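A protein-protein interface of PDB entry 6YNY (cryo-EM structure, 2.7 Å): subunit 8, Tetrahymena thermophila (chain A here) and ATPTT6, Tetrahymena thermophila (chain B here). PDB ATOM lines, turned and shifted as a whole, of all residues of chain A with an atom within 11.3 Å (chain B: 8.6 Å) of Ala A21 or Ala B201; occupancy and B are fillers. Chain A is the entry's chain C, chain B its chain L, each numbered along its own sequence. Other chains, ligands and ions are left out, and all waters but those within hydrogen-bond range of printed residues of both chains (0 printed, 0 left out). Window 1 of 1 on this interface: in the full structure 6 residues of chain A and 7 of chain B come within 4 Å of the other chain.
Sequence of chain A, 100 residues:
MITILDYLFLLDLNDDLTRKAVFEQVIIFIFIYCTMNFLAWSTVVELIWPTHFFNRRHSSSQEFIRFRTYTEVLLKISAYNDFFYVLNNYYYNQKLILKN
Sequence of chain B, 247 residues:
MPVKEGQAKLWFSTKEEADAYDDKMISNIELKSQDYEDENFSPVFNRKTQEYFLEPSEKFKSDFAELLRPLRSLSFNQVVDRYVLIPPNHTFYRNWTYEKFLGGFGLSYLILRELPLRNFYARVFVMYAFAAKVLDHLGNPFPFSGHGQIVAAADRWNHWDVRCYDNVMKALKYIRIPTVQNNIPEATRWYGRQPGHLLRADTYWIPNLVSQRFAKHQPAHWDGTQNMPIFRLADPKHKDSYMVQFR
Of chain B, only Leu B199 and Ala B201 come within 4 Å of Ala A21.
Ala B201 touches three residues of chain A.
Of chain A, only Ala A21 and Glu A24 come within 4 Å of Leu B199.
Printed residues of chain B within 4 Å of Lys A20: Ala B201 and His B217.
Of the printed residues of chain A, Phe B231 touches Leu A17 (3.3 Å).
Of the printed residues of chain B, Gln A25 touches Ala B201, Asp B202, Thr B203 and Tyr B204.
Asp A12 touches none of the printed residues of chain B.
The nearest residue of chain A that does not touch Ala B201 is Val A22 (4.1 Å).
The nearest printed residue of chain A that does not touch Phe B231 is Thr A18 (5.2 Å).
Among the printed residues, merely in contact across the chains: Arg A19 with His B217 (2.9 Å), Ala A21 with Ala B201 (3.1 Å), Lys A20 with Ala B201 (3.3 Å), Leu A17 with Phe B231 (3.3 Å), Lys A20 with His B217 (3.6 Å), Gln A25 with Asp B202 (3.7 Å), Gln A25 with Tyr B204 (3.7 Å), Glu A24 with Leu B199 (3.7 Å) and Ala A21 with Leu B199 (3.9 Å).
N of Ala A21 is in hydrogen-bond range of O of Asp A16 (3.1 Å).
OD1 of Asp B202 lies within hydrogen-bond range of N of Tyr B204, 3.2 Å away.
The side-chain amide nitrogen (ND2) of Asn B208 is in hydrogen-bond range of the side-chain carboxylate (OD2) of Asp B202.
The backbone carbonyl oxygen (O) of Asp A15 lies within hydrogen-bond range of the guanidinium group (NH1) of Arg A19 (3.2 Å).
N of Trp B205 sits close to OD2 of Asp B202 (3.1 Å).
OD2 of Asp A12 lies within salt-bridge range of NH1 of Arg A19, at 2.9 Å.
Of the 16 printed residues of chain B, 7 touch a printed residue of chain A.
Hydrophobic or aromatic side chains of chain B that line the printed part of chain A: Leu B199, Ala B201, Tyr B204, His B217 and Phe B231.
Along chain B the printed residues that touch a printed residue of chain A span positions 199 to 231.
Hydrophobic or aromatic side chains of chain A that line the printed part of chain B: Ala A21.
Along chain A the printed residues that touch a printed residue of chain B span positions 17 to 25.
OE1 of Gln A25 is in hydrogen-bond range of OG1 of Thr B203 (2.8 Å).
O of Ala B201 sits at hydrogen-bond distance from NE2 of Gln A25, 3.0 Å away.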
ATOM      1  N   LEU A  10      31.387 -28.053  13.034  1.00  0.00           N
ATOM      2  CA  LEU A  10      30.915 -28.363  14.375  1.00  0.00           C
ATOM      3  C   LEU A  10      32.041 -28.373  15.396  1.00  0.00           C
ATOM      4  O   LEU A  10      31.770 -28.313  16.600  1.00  0.00           O
ATOM      5  CB  LEU A  10      30.216 -29.718  14.373  1.00  0.00           C
ATOM      6  CG  LEU A  10      29.081 -29.867  13.364  1.00  0.00           C
ATOM      7  CD1 LEU A  10      28.556 -31.277  13.374  1.00  0.00           C
ATOM      8  CD2 LEU A  10      27.974 -28.889  13.671  1.00  0.00           C
ATOM      9  N   ASP A  12      34.009 -26.034  15.957  1.00  0.00           N
ATOM     10  CA  ASP A  12      34.296 -24.665  16.351  1.00  0.00           C
ATOM     11  C   ASP A  12      33.665 -24.340  17.696  1.00  0.00           C
ATOM     12  O   ASP A  12      32.489 -24.635  17.933  1.00  0.00           O
ATOM     13  CB  ASP A  12      33.786 -23.698  15.288  1.00  0.00           C
ATOM     14  CG  ASP A  12      34.112 -22.256  15.609  1.00  0.00           C
ATOM     15  OD1 ASP A  12      35.308 -21.900  15.598  1.00  0.00           O
ATOM     16  OD2 ASP A  12      33.174 -21.477  15.867  1.00  0.00           O
ATOM     17  N   LEU A  13      34.457 -23.730  18.574  1.00  0.00           N
ATOM     18  CA  LEU A  13      33.960 -23.167  19.817  1.00  0.00           C
ATOM     19  C   LEU A  13      34.344 -21.711  20.005  1.00  0.00           C
ATOM     20  O   LEU A  13      33.872 -21.088  20.961  1.00  0.00           O
ATOM     21  CB  LEU A  13      34.460 -23.974  21.021  1.00  0.00           C
ATOM     22  CG  LEU A  13      33.962 -25.417  21.098  1.00  0.00           C
ATOM     23  CD1 LEU A  13      34.599 -26.126  22.259  1.00  0.00           C
ATOM     24  CD2 LEU A  13      32.449 -25.470  21.221  1.00  0.00           C
ATOM     25  N   ASN A  14      35.179 -21.147  19.129  1.00  0.00           N
ATOM     26  CA  ASN A  14      35.511 -19.733  19.230  1.00  0.00           C
ATOM     27  C   ASN A  14      34.301 -18.863  18.929  1.00  0.00           C
ATOM     28  O   ASN A  14      34.109 -17.815  19.555  1.00  0.00           O
ATOM     29  CB  ASN A  14      36.644 -19.388  18.268  1.00  0.00           C
ATOM     30  CG  ASN A  14      37.930 -20.092  18.598  1.00  0.00           C
ATOM     31  OD1 ASN A  14      38.191 -20.445  19.747  1.00  0.00           O
ATOM     32  ND2 ASN A  14      38.753 -20.298  17.584  1.00  0.00           N
ATOM     33  N   ASP A  15      33.478 -19.281  17.970  1.00  0.00           N
ATOM     34  CA  ASP A  15      32.343 -18.497  17.505  1.00  0.00           C
ATOM     35  C   ASP A  15      31.022 -19.214  17.739  1.00  0.00           C
ATOM     36  O   ASP A  15      30.036 -18.931  17.053  1.00  0.00           O
ATOM     37  CB  ASP A  15      32.514 -18.164  16.024  1.00  0.00           C
ATOM     38  CG  ASP A  15      33.781 -17.385  15.747  1.00  0.00           C
ATOM     39  OD1 ASP A  15      34.070 -16.431  16.500  1.00  0.00           O
ATOM     40  OD2 ASP A  15      34.496 -17.734  14.785  1.00  0.00           O
ATOM     41  N   ASP A  16      30.979 -20.140  18.696  1.00  0.00           N
ATOM     42  CA  ASP A  16      29.731 -20.823  19.001  1.00  0.00           C
ATOM     43  C   ASP A  16      28.678 -19.868  19.539  1.00  0.00           C
ATOM     44  O   ASP A  16      27.484 -20.174  19.462  1.00  0.00           O
ATOM     45  CB  ASP A  16      29.974 -21.949  20.005  1.00  0.00           C
ATOM     46  CG  ASP A  16      28.759 -22.830  20.193  1.00  0.00           C
ATOM     47  OD1 ASP A  16      27.847 -22.773  19.345  1.00  0.00           O
ATOM     48  OD2 ASP A  16      28.712 -23.575  21.193  1.00  0.00           O
ATOM     49  N   LEU A  17      29.087 -18.720  20.078  1.00  0.00           N
ATOM     50  CA  LEU A  17      28.115 -17.743  20.545  1.00  0.00           C
ATOM     51  C   LEU A  17      27.328 -17.119  19.405  1.00  0.00           C
ATOM     52  O   LEU A  17      26.374 -16.381  19.665  1.00  0.00           O
ATOM     53  CB  LEU A  17      28.805 -16.647  21.360  1.00  0.00           C
ATOM     54  CG  LEU A  17      29.838 -15.747  20.684  1.00  0.00           C
ATOM     55  CD1 LEU A  17      29.178 -14.652  19.888  1.00  0.00           C
ATOM     56  CD2 LEU A  17      30.750 -15.150  21.729  1.00  0.00           C
ATOM     57  N   THR A  18      27.706 -17.390  18.157  1.00  0.00           N
ATOM     58  CA  THR A  18      26.969 -16.877  17.017  1.00  0.00           C
ATOM     59  C   THR A  18      25.821 -17.781  16.598  1.00  0.00           C
ATOM     60  O   THR A  18      24.951 -17.334  15.844  1.00  0.00           O
ATOM     61  CB  THR A  18      27.901 -16.674  15.817  1.00  0.00           C
ATOM     62  OG1 THR A  18      28.485 -17.924  15.437  1.00  0.00           O
ATOM     63  CG2 THR A  18      28.993 -15.701  16.159  1.00  0.00           C
ATOM     64  N   ARG A  19      25.796 -19.035  17.054  1.00  0.00           N
ATOM     65  CA  ARG A  19      24.754 -19.967  16.646  1.00  0.00           C
ATOM     66  C   ARG A  19      23.835 -20.376  17.790  1.00  0.00           C
ATOM     67  O   ARG A  19      22.630 -20.127  17.719  1.00  0.00           O
ATOM     68  CB  ARG A  19      25.394 -21.215  16.027  1.00  0.00           C
ATOM     69  CG  ARG A  19      26.110 -20.984  14.710  1.00  0.00           C
ATOM     70  CD  ARG A  19      27.612 -21.074  14.845  1.00  0.00           C
ATOM     71  NE  ARG A  19      28.037 -22.331  15.450  1.00  0.00           N
ATOM     72  CZ  ARG A  19      29.298 -22.626  15.749  1.00  0.00           C
ATOM     73  NH1 ARG A  19      30.269 -21.763  15.490  1.00  0.00           N
ATOM     74  NH2 ARG A  19      29.589 -23.792  16.306  1.00  0.00           N
ATOM     75  N   LYS A  20      24.360 -20.990  18.847  1.00  0.00           N
ATOM     76  CA  LYS A  20      23.506 -21.390  19.963  1.00  0.00           C
ATOM     77  C   LYS A  20      24.077 -21.049  21.331  1.00  0.00           C
ATOM     78  O   LYS A  20      23.323 -20.636  22.215  1.00  0.00           O
ATOM     79  CB  LYS A  20      23.228 -22.890  19.892  1.00  0.00           C
ATOM     80  CG  LYS A  20      22.586 -23.341  18.599  1.00  0.00           C
ATOM     81  CD  LYS A  20      22.167 -24.796  18.670  1.00  0.00           C
ATOM     82  CE  LYS A  20      21.705 -25.311  17.324  1.00  0.00           C
ATOM     83  NZ  LYS A  20      20.603 -24.495  16.778  1.00  0.00           N
ATOM     84  N   ALA A  21      25.384 -21.212  21.529  1.00  0.00           N
ATOM     85  CA  ALA A  21      26.010 -21.032  22.838  1.00  0.00           C
ATOM     86  C   ALA A  21      25.426 -21.992  23.872  1.00  0.00           C
ATOM     87  O   ALA A  21      25.285 -21.655  25.049  1.00  0.00           O
ATOM     88  CB  ALA A  21      25.885 -19.588  23.317  1.00  0.00           C
ATOM     89  N   VAL A  22      25.093 -23.204  23.434  1.00  0.00           N
ATOM     90  CA  VAL A  22      24.497 -24.200  24.308  1.00  0.00           C
ATOM     91  C   VAL A  22      25.477 -25.300  24.699  1.00  0.00           C
ATOM     92  O   VAL A  22      25.377 -25.829  25.812  1.00  0.00           O
ATOM     93  CB  VAL A  22      23.238 -24.806  23.654  1.00  0.00           C
ATOM     94  CG1 VAL A  22      22.694 -25.926  24.503  1.00  0.00           C
ATOM     95  CG2 VAL A  22      22.185 -23.746  23.452  1.00  0.00           C
ATOM     96  N   PHE A  23      26.414 -25.660  23.825  1.00  0.00           N
ATOM     97  CA  PHE A  23      27.364 -26.720  24.142  1.00  0.00           C
ATOM     98  C   PHE A  23      28.109 -26.426  25.437  1.00  0.00           C
ATOM     99  O   PHE A  23      28.304 -27.321  26.267  1.00  0.00           O
ATOM    100  CB  PHE A  23      28.346 -26.888  22.984  1.00  0.00           C
ATOM    101  CG  PHE A  23      29.386 -27.939  23.214  1.00  0.00           C
ATOM    102  CD1 PHE A  23      29.153 -29.250  22.851  1.00  0.00           C
ATOM    103  CD2 PHE A  23      30.602 -27.616  23.782  1.00  0.00           C
ATOM    104  CE1 PHE A  23      30.108 -30.214  23.056  1.00  0.00           C
ATOM    105  CE2 PHE A  23      31.557 -28.578  23.990  1.00  0.00           C
ATOM    106  CZ  PHE A  23      31.310 -29.879  23.627  1.00  0.00           C
ATOM    107  N   GLU A  24      28.523 -25.175  25.633  1.00  0.00           N
ATOM    108  CA  GLU A  24      29.323 -24.821  26.799  1.00  0.00           C
ATOM    109  C   GLU A  24      28.603 -25.082  28.115  1.00  0.00           C
ATOM    110  O   GLU A  24      29.263 -25.164  29.156  1.00  0.00           O
ATOM    111  CB  GLU A  24      29.744 -23.353  26.711  1.00  0.00           C
ATOM    112  CG  GLU A  24      28.607 -22.378  26.493  1.00  0.00           C
ATOM    113  CD  GLU A  24      29.085 -20.947  26.369  1.00  0.00           C
ATOM    114  OE1 GLU A  24      30.313 -20.733  26.330  1.00  0.00           O
ATOM    115  OE2 GLU A  24      28.234 -20.036  26.310  1.00  0.00           O
ATOM    116  N   GLN A  25      27.279 -25.222  28.102  1.00  0.00           N
ATOM    117  CA  GLN A  25      26.516 -25.445  29.323  1.00  0.00           C
ATOM    118  C   GLN A  25      26.022 -26.870  29.488  1.00  0.00           C
ATOM    119  O   GLN A  25      25.865 -27.326  30.621  1.00  0.00           O
ATOM    120  CB  GLN A  25      25.306 -24.509  29.372  1.00  0.00           C
ATOM    121  CG  GLN A  25      25.649 -23.058  29.596  1.00  0.00           C
ATOM    122  CD  GLN A  25      24.426 -22.190  29.746  1.00  0.00           C
ATOM    123  OE1 GLN A  25      23.461 -22.567  30.408  1.00  0.00           O
ATOM    124  NE2 GLN A  25      24.453 -21.023  29.123  1.00  0.00           N
ATOM    125  N   VAL A  26      25.771 -27.584  28.392  1.00  0.00           N
ATOM    126  CA  VAL A  26      25.188 -28.915  28.494  1.00  0.00           C
ATOM    127  C   VAL A  26      26.222 -29.925  28.969  1.00  0.00           C
ATOM    128  O   VAL A  26      25.905 -30.842  29.735  1.00  0.00           O
ATOM    129  CB  VAL A  26      24.567 -29.323  27.148  1.00  0.00           C
ATOM    130  CG1 VAL A  26      24.104 -30.755  27.194  1.00  0.00           C
ATOM    131  CG2 VAL A  26      23.414 -28.418  26.818  1.00  0.00           C
ATOM    132  N   ILE A  27      27.471 -29.781  28.525  1.00  0.00           N
ATOM    133  CA  ILE A  27      28.497 -30.742  28.915  1.00  0.00           C
ATOM    134  C   ILE A  27      28.767 -30.673  30.409  1.00  0.00           C
ATOM    135  O   ILE A  27      29.223 -31.653  31.008  1.00  0.00           O
ATOM    136  CB  ILE A  27      29.784 -30.519  28.102  1.00  0.00           C
ATOM    137  CG1 ILE A  27      30.319 -29.109  28.318  1.00  0.00           C
ATOM    138  CG2 ILE A  27      29.527 -30.764  26.639  1.00  0.00           C
ATOM    139  CD1 ILE A  27      31.630 -28.873  27.656  1.00  0.00           C
ATOM    140  N   ILE A  28      28.503 -29.527  31.037  1.00  0.00           N
ATOM    141  CA  ILE A  28      28.619 -29.439  32.488  1.00  0.00           C
ATOM    142  C   ILE A  28      27.707 -30.462  33.146  1.00  0.00           C
ATOM    143  O   ILE A  28      28.113 -31.191  34.057  1.00  0.00           O
ATOM    144  CB  ILE A  28      28.298 -28.011  32.962  1.00  0.00           C
ATOM    145  CG1 ILE A  28      29.382 -27.047  32.492  1.00  0.00           C
ATOM    146  CG2 ILE A  28      28.158 -27.974  34.472  1.00  0.00           C
ATOM    147  CD1 ILE A  28      29.048 -25.601  32.726  1.00  0.00           C
ATOM    148  N   LEU B 198      24.169 -10.037  26.953  1.00  0.00           N
ATOM    149  CA  LEU B 198      24.105 -11.269  27.719  1.00  0.00           C
ATOM    150  C   LEU B 198      23.448 -12.344  26.869  1.00  0.00           C
ATOM    151  O   LEU B 198      22.399 -12.109  26.265  1.00  0.00           O
ATOM    152  CB  LEU B 198      23.333 -11.047  29.018  1.00  0.00           C
ATOM    153  CG  LEU B 198      23.237 -12.195  30.015  1.00  0.00           C
ATOM    154  CD1 LEU B 198      24.590 -12.551  30.556  1.00  0.00           C
ATOM    155  CD2 LEU B 198      22.307 -11.812  31.135  1.00  0.00           C
ATOM    156  N   LEU B 199      24.069 -13.517  26.822  1.00  0.00           N
ATOM    157  CA  LEU B 199      23.592 -14.585  25.958  1.00  0.00           C
ATOM    158  C   LEU B 199      22.214 -15.068  26.396  1.00  0.00           C
ATOM    159  O   LEU B 199      21.889 -15.102  27.584  1.00  0.00           O
ATOM    160  CB  LEU B 199      24.581 -15.749  25.967  1.00  0.00           C
ATOM    161  CG  LEU B 199      25.953 -15.461  25.366  1.00  0.00           C
ATOM    162  CD1 LEU B 199      26.898 -16.605  25.631  1.00  0.00           C
ATOM    163  CD2 LEU B 199      25.843 -15.210  23.883  1.00  0.00           C
ATOM    164  N   ARG B 200      21.399 -15.444  25.408  1.00  0.00           N
ATOM    165  CA  ARG B 200      20.092 -16.018  25.707  1.00  0.00           C
ATOM    166  C   ARG B 200      20.218 -17.444  26.222  1.00  0.00           C
ATOM    167  O   ARG B 200      19.442 -17.867  27.085  1.00  0.00           O
ATOM    168  CB  ARG B 200      19.207 -15.997  24.463  1.00  0.00           C
ATOM    169  CG  ARG B 200      18.796 -14.627  23.984  1.00  0.00           C
ATOM    170  CD  ARG B 200      17.918 -13.916  24.981  1.00  0.00           C
ATOM    171  NE  ARG B 200      16.744 -14.694  25.365  1.00  0.00           N
ATOM    172  CZ  ARG B 200      15.575 -14.660  24.735  1.00  0.00           C
ATOM    173  NH1 ARG B 200      14.572 -15.402  25.170  1.00  0.00           N
ATOM    174  NH2 ARG B 200      15.401 -13.889  23.675  1.00  0.00           N
ATOM    175  N   ALA B 201      21.181 -18.196  25.702  1.00  0.00           N
ATOM    176  CA  ALA B 201      21.347 -19.587  26.095  1.00  0.00           C
ATOM    177  C   ALA B 201      21.470 -19.701  27.603  1.00  0.00           C
ATOM    178  O   ALA B 201      22.379 -19.127  28.207  1.00  0.00           O
ATOM    179  CB  ALA B 201      22.579 -20.176  25.413  1.00  0.00           C
ATOM    180  N   ASP B 202      20.553 -20.449  28.205  1.00  0.00           N
ATOM    181  CA  ASP B 202      20.491 -20.556  29.658  1.00  0.00           C
ATOM    182  C   ASP B 202      19.864 -21.891  30.025  1.00  0.00           C
ATOM    183  O   ASP B 202      18.676 -22.111  29.775  1.00  0.00           O
ATOM    184  CB  ASP B 202      19.695 -19.399  30.249  1.00  0.00           C
ATOM    185  CG  ASP B 202      19.410 -19.583  31.717  1.00  0.00           C
ATOM    186  OD1 ASP B 202      20.372 -19.714  32.500  1.00  0.00           O
ATOM    187  OD2 ASP B 202      18.221 -19.587  32.090  1.00  0.00           O
ATOM    188  N   THR B 203      20.664 -22.775  30.610  1.00  0.00           N
ATOM    189  CA  THR B 203      20.188 -24.042  31.137  1.00  0.00           C
ATOM    190  C   THR B 203      19.994 -24.002  32.644  1.00  0.00           C
ATOM    191  O   THR B 203      19.581 -25.004  33.232  1.00  0.00           O
ATOM    192  CB  THR B 203      21.165 -25.163  30.779  1.00  0.00           C
ATOM    193  OG1 THR B 203      22.427 -24.925  31.414  1.00  0.00           O
ATOM    194  CG2 THR B 203      21.365 -25.233  29.283  1.00  0.00           C
ATOM    195  N   TYR B 204      20.279 -22.866  33.276  1.00  0.00           N
ATOM    196  CA  TYR B 204      20.167 -22.732  34.719  1.00  0.00           C
ATOM    197  C   TYR B 204      18.754 -22.399  35.170  1.00  0.00           C
ATOM    198  O   TYR B 204      18.400 -22.682  36.319  1.00  0.00           O
ATOM    199  CB  TYR B 204      21.140 -21.658  35.199  1.00  0.00           C
ATOM    200  CG  TYR B 204      22.556 -21.890  34.735  1.00  0.00           C
ATOM    201  CD1 TYR B 204      23.191 -23.100  34.962  1.00  0.00           C
ATOM    202  CD2 TYR B 204      23.250 -20.907  34.050  1.00  0.00           C
ATOM    203  CE1 TYR B 204      24.479 -23.318  34.536  1.00  0.00           C
ATOM    204  CE2 TYR B 204      24.539 -21.117  33.620  1.00  0.00           C
ATOM    205  CZ  TYR B 204      25.148 -22.325  33.865  1.00  0.00           C
ATOM    206  OH  TYR B 204      26.435 -22.542  33.437  1.00  0.00           O
ATOM    207  N   TRP B 205      17.950 -21.801  34.300  1.00  0.00           N
ATOM    208  CA  TRP B 205      16.544 -21.534  34.564  1.00  0.00           C
ATOM    209  C   TRP B 205      15.718 -22.578  33.824  1.00  0.00           C
ATOM    210  O   TRP B 205      15.750 -22.639  32.591  1.00  0.00           O
ATOM    211  CB  TRP B 205      16.177 -20.126  34.104  1.00  0.00           C
ATOM    212  CG  TRP B 205      15.150 -19.434  34.928  1.00  0.00           C
ATOM    213  CD1 TRP B 205      15.065 -19.412  36.284  1.00  0.00           C
ATOM    214  CD2 TRP B 205      14.060 -18.650  34.444  1.00  0.00           C
ATOM    215  NE1 TRP B 205      13.989 -18.662  36.676  1.00  0.00           N
ATOM    216  CE2 TRP B 205      13.353 -18.183  35.563  1.00  0.00           C
ATOM    217  CE3 TRP B 205      13.612 -18.299  33.170  1.00  0.00           C
ATOM    218  CZ2 TRP B 205      12.223 -17.386  35.449  1.00  0.00           C
ATOM    219  CZ3 TRP B 205      12.492 -17.508  33.060  1.00  0.00           C
ATOM    220  CH2 TRP B 205      11.810 -17.060  34.190  1.00  0.00           C
ATOM    221  N   ASN B 208      13.607 -21.923  30.614  1.00  0.00           N
ATOM    222  CA  ASN B 208      14.361 -21.796  29.375  1.00  0.00           C
ATOM    223  C   ASN B 208      14.977 -23.118  28.958  1.00  0.00           C
ATOM    224  O   ASN B 208      15.125 -23.379  27.761  1.00  0.00           O
ATOM    225  CB  ASN B 208      15.447 -20.739  29.528  1.00  0.00           C
ATOM    226  CG  ASN B 208      14.884 -19.360  29.746  1.00  0.00           C
ATOM    227  OD1 ASN B 208      13.765 -19.061  29.337  1.00  0.00           O
ATOM    228  ND2 ASN B 208      15.656 -18.507  30.394  1.00  0.00           N
ATOM    229  N   LEU B 209      15.340 -23.957  29.927  1.00  0.00           N
ATOM    230  CA  LEU B 209      15.851 -25.281  29.606  1.00  0.00           C
ATOM    231  C   LEU B 209      14.838 -26.083  28.802  1.00  0.00           C
ATOM    232  O   LEU B 209      15.220 -26.949  28.009  1.00  0.00           O
ATOM    233  CB  LEU B 209      16.217 -26.012  30.893  1.00  0.00           C
ATOM    234  CG  LEU B 209      16.789 -27.422  30.751  1.00  0.00           C
ATOM    235  CD1 LEU B 209      18.067 -27.405  29.948  1.00  0.00           C
ATOM    236  CD2 LEU B 209      17.024 -28.019  32.117  1.00  0.00           C
ATOM    237  N   GLN B 212      13.757 -23.258  25.310  1.00  0.00           N
ATOM    238  CA  GLN B 212      14.778 -23.041  24.294  1.00  0.00           C
ATOM    239  C   GLN B 212      15.040 -24.274  23.445  1.00  0.00           C
ATOM    240  O   GLN B 212      15.769 -24.177  22.452  1.00  0.00           O
ATOM    241  CB  GLN B 212      16.074 -22.572  24.948  1.00  0.00           C
ATOM    242  CG  GLN B 212      15.967 -21.204  25.583  1.00  0.00           C
ATOM    243  CD  GLN B 212      17.282 -20.708  26.124  1.00  0.00           C
ATOM    244  OE1 GLN B 212      18.203 -21.485  26.365  1.00  0.00           O
ATOM    245  NE2 GLN B 212      17.382 -19.403  26.312  1.00  0.00           N
ATOM    246  N   ARG B 213      14.476 -25.425  23.807  1.00  0.00           N
ATOM    247  CA  ARG B 213      14.563 -26.604  22.961  1.00  0.00           C
ATOM    248  C   ARG B 213      13.641 -26.515  21.757  1.00  0.00           C
ATOM    249  O   ARG B 213      13.897 -27.175  20.745  1.00  0.00           O
ATOM    250  CB  ARG B 213      14.221 -27.854  23.769  1.00  0.00           C
ATOM    251  CG  ARG B 213      15.002 -28.016  25.056  1.00  0.00           C
ATOM    252  CD  ARG B 213      16.453 -28.360  24.824  1.00  0.00           C
ATOM    253  NE  ARG B 213      17.240 -27.235  24.333  1.00  0.00           N
ATOM    254  CZ  ARG B 213      17.650 -26.224  25.089  1.00  0.00           C
ATOM    255  NH1 ARG B 213      17.340 -26.184  26.375  1.00  0.00           N
ATOM    256  NH2 ARG B 213      18.365 -25.247  24.559  1.00  0.00           N
ATOM    257  N   HIS B 217      16.370 -20.714  15.839  1.00  0.00           N
ATOM    258  CA  HIS B 217      17.460 -19.765  15.653  1.00  0.00           C
ATOM    259  C   HIS B 217      17.388 -19.207  14.240  1.00  0.00           C
ATOM    260  O   HIS B 217      17.710 -19.902  13.272  1.00  0.00           O
ATOM    261  CB  HIS B 217      18.804 -20.435  15.909  1.00  0.00           C
ATOM    262  CG  HIS B 217      19.021 -20.826  17.334  1.00  0.00           C
ATOM    263  ND1 HIS B 217      18.386 -21.898  17.918  1.00  0.00           N
ATOM    264  CD2 HIS B 217      19.800 -20.280  18.295  1.00  0.00           C
ATOM    265  CE1 HIS B 217      18.767 -21.999  19.178  1.00  0.00           C
ATOM    266  NE2 HIS B 217      19.626 -21.029  19.432  1.00  0.00           N
ATOM    267  N   ILE B 230      20.935  -8.742  19.628  1.00  0.00           N
ATOM    268  CA  ILE B 230      20.419 -10.042  19.211  1.00  0.00           C
ATOM    269  C   ILE B 230      20.334 -11.024  20.364  1.00  0.00           C
ATOM    270  O   ILE B 230      19.774 -12.115  20.200  1.00  0.00           O
ATOM    271  CB  ILE B 230      21.285 -10.626  18.081  1.00  0.00           C
ATOM    272  CG1 ILE B 230      22.701 -10.908  18.574  1.00  0.00           C
ATOM    273  CG2 ILE B 230      21.319  -9.677  16.916  1.00  0.00           C
ATOM    274  CD1 ILE B 230      23.658 -11.256  17.482  1.00  0.00           C
ATOM    275  N   PHE B 231      20.874 -10.670  21.521  1.00  0.00           N
ATOM    276  CA  PHE B 231      20.707 -11.422  22.751  1.00  0.00           C
ATOM    277  C   PHE B 231      20.003 -10.527  23.763  1.00  0.00           C
ATOM    278  O   PHE B 231      19.556  -9.423  23.446  1.00  0.00           O
ATOM    279  CB  PHE B 231      22.049 -11.910  23.296  1.00  0.00           C
ATOM    280  CG  PHE B 231      22.943 -12.515  22.265  1.00  0.00           C
ATOM    281  CD1 PHE B 231      22.562 -13.643  21.572  1.00  0.00           C
ATOM    282  CD2 PHE B 231      24.179 -11.962  22.002  1.00  0.00           C
ATOM    283  CE1 PHE B 231      23.391 -14.197  20.629  1.00  0.00           C
ATOM    284  CE2 PHE B 231      25.008 -12.513  21.064  1.00  0.00           C
ATOM    285  CZ  PHE B 231      24.616 -13.629  20.377  1.00  0.00           C
ATOM    286  N   ARG B 232      19.897 -11.016  24.990  1.00  0.00           N
ATOM    287  CA  ARG B 232      19.384 -10.191  26.064  1.00  0.00           C
ATOM    288  C   ARG B 232      20.486  -9.275  26.586  1.00  0.00           C
ATOM    289  O   ARG B 232      21.654  -9.378  26.204  1.00  0.00           O
ATOM    290  CB  ARG B 232      18.815 -11.057  27.184  1.00  0.00           C
ATOM    291  CG  ARG B 232      19.760 -12.094  27.720  1.00  0.00           C
ATOM    292  CD  ARG B 232      19.128 -12.858  28.839  1.00  0.00           C
ATOM    293  NE  ARG B 232      19.999 -13.910  29.340  1.00  0.00           N
ATOM    294  CZ  ARG B 232      19.752 -14.624  30.430  1.00  0.00           C
ATOM    295  NH1 ARG B 232      18.665 -14.396  31.143  1.00  0.00           N
ATOM    296  NH2 ARG B 232      20.600 -15.561  30.809  1.00  0.00           N
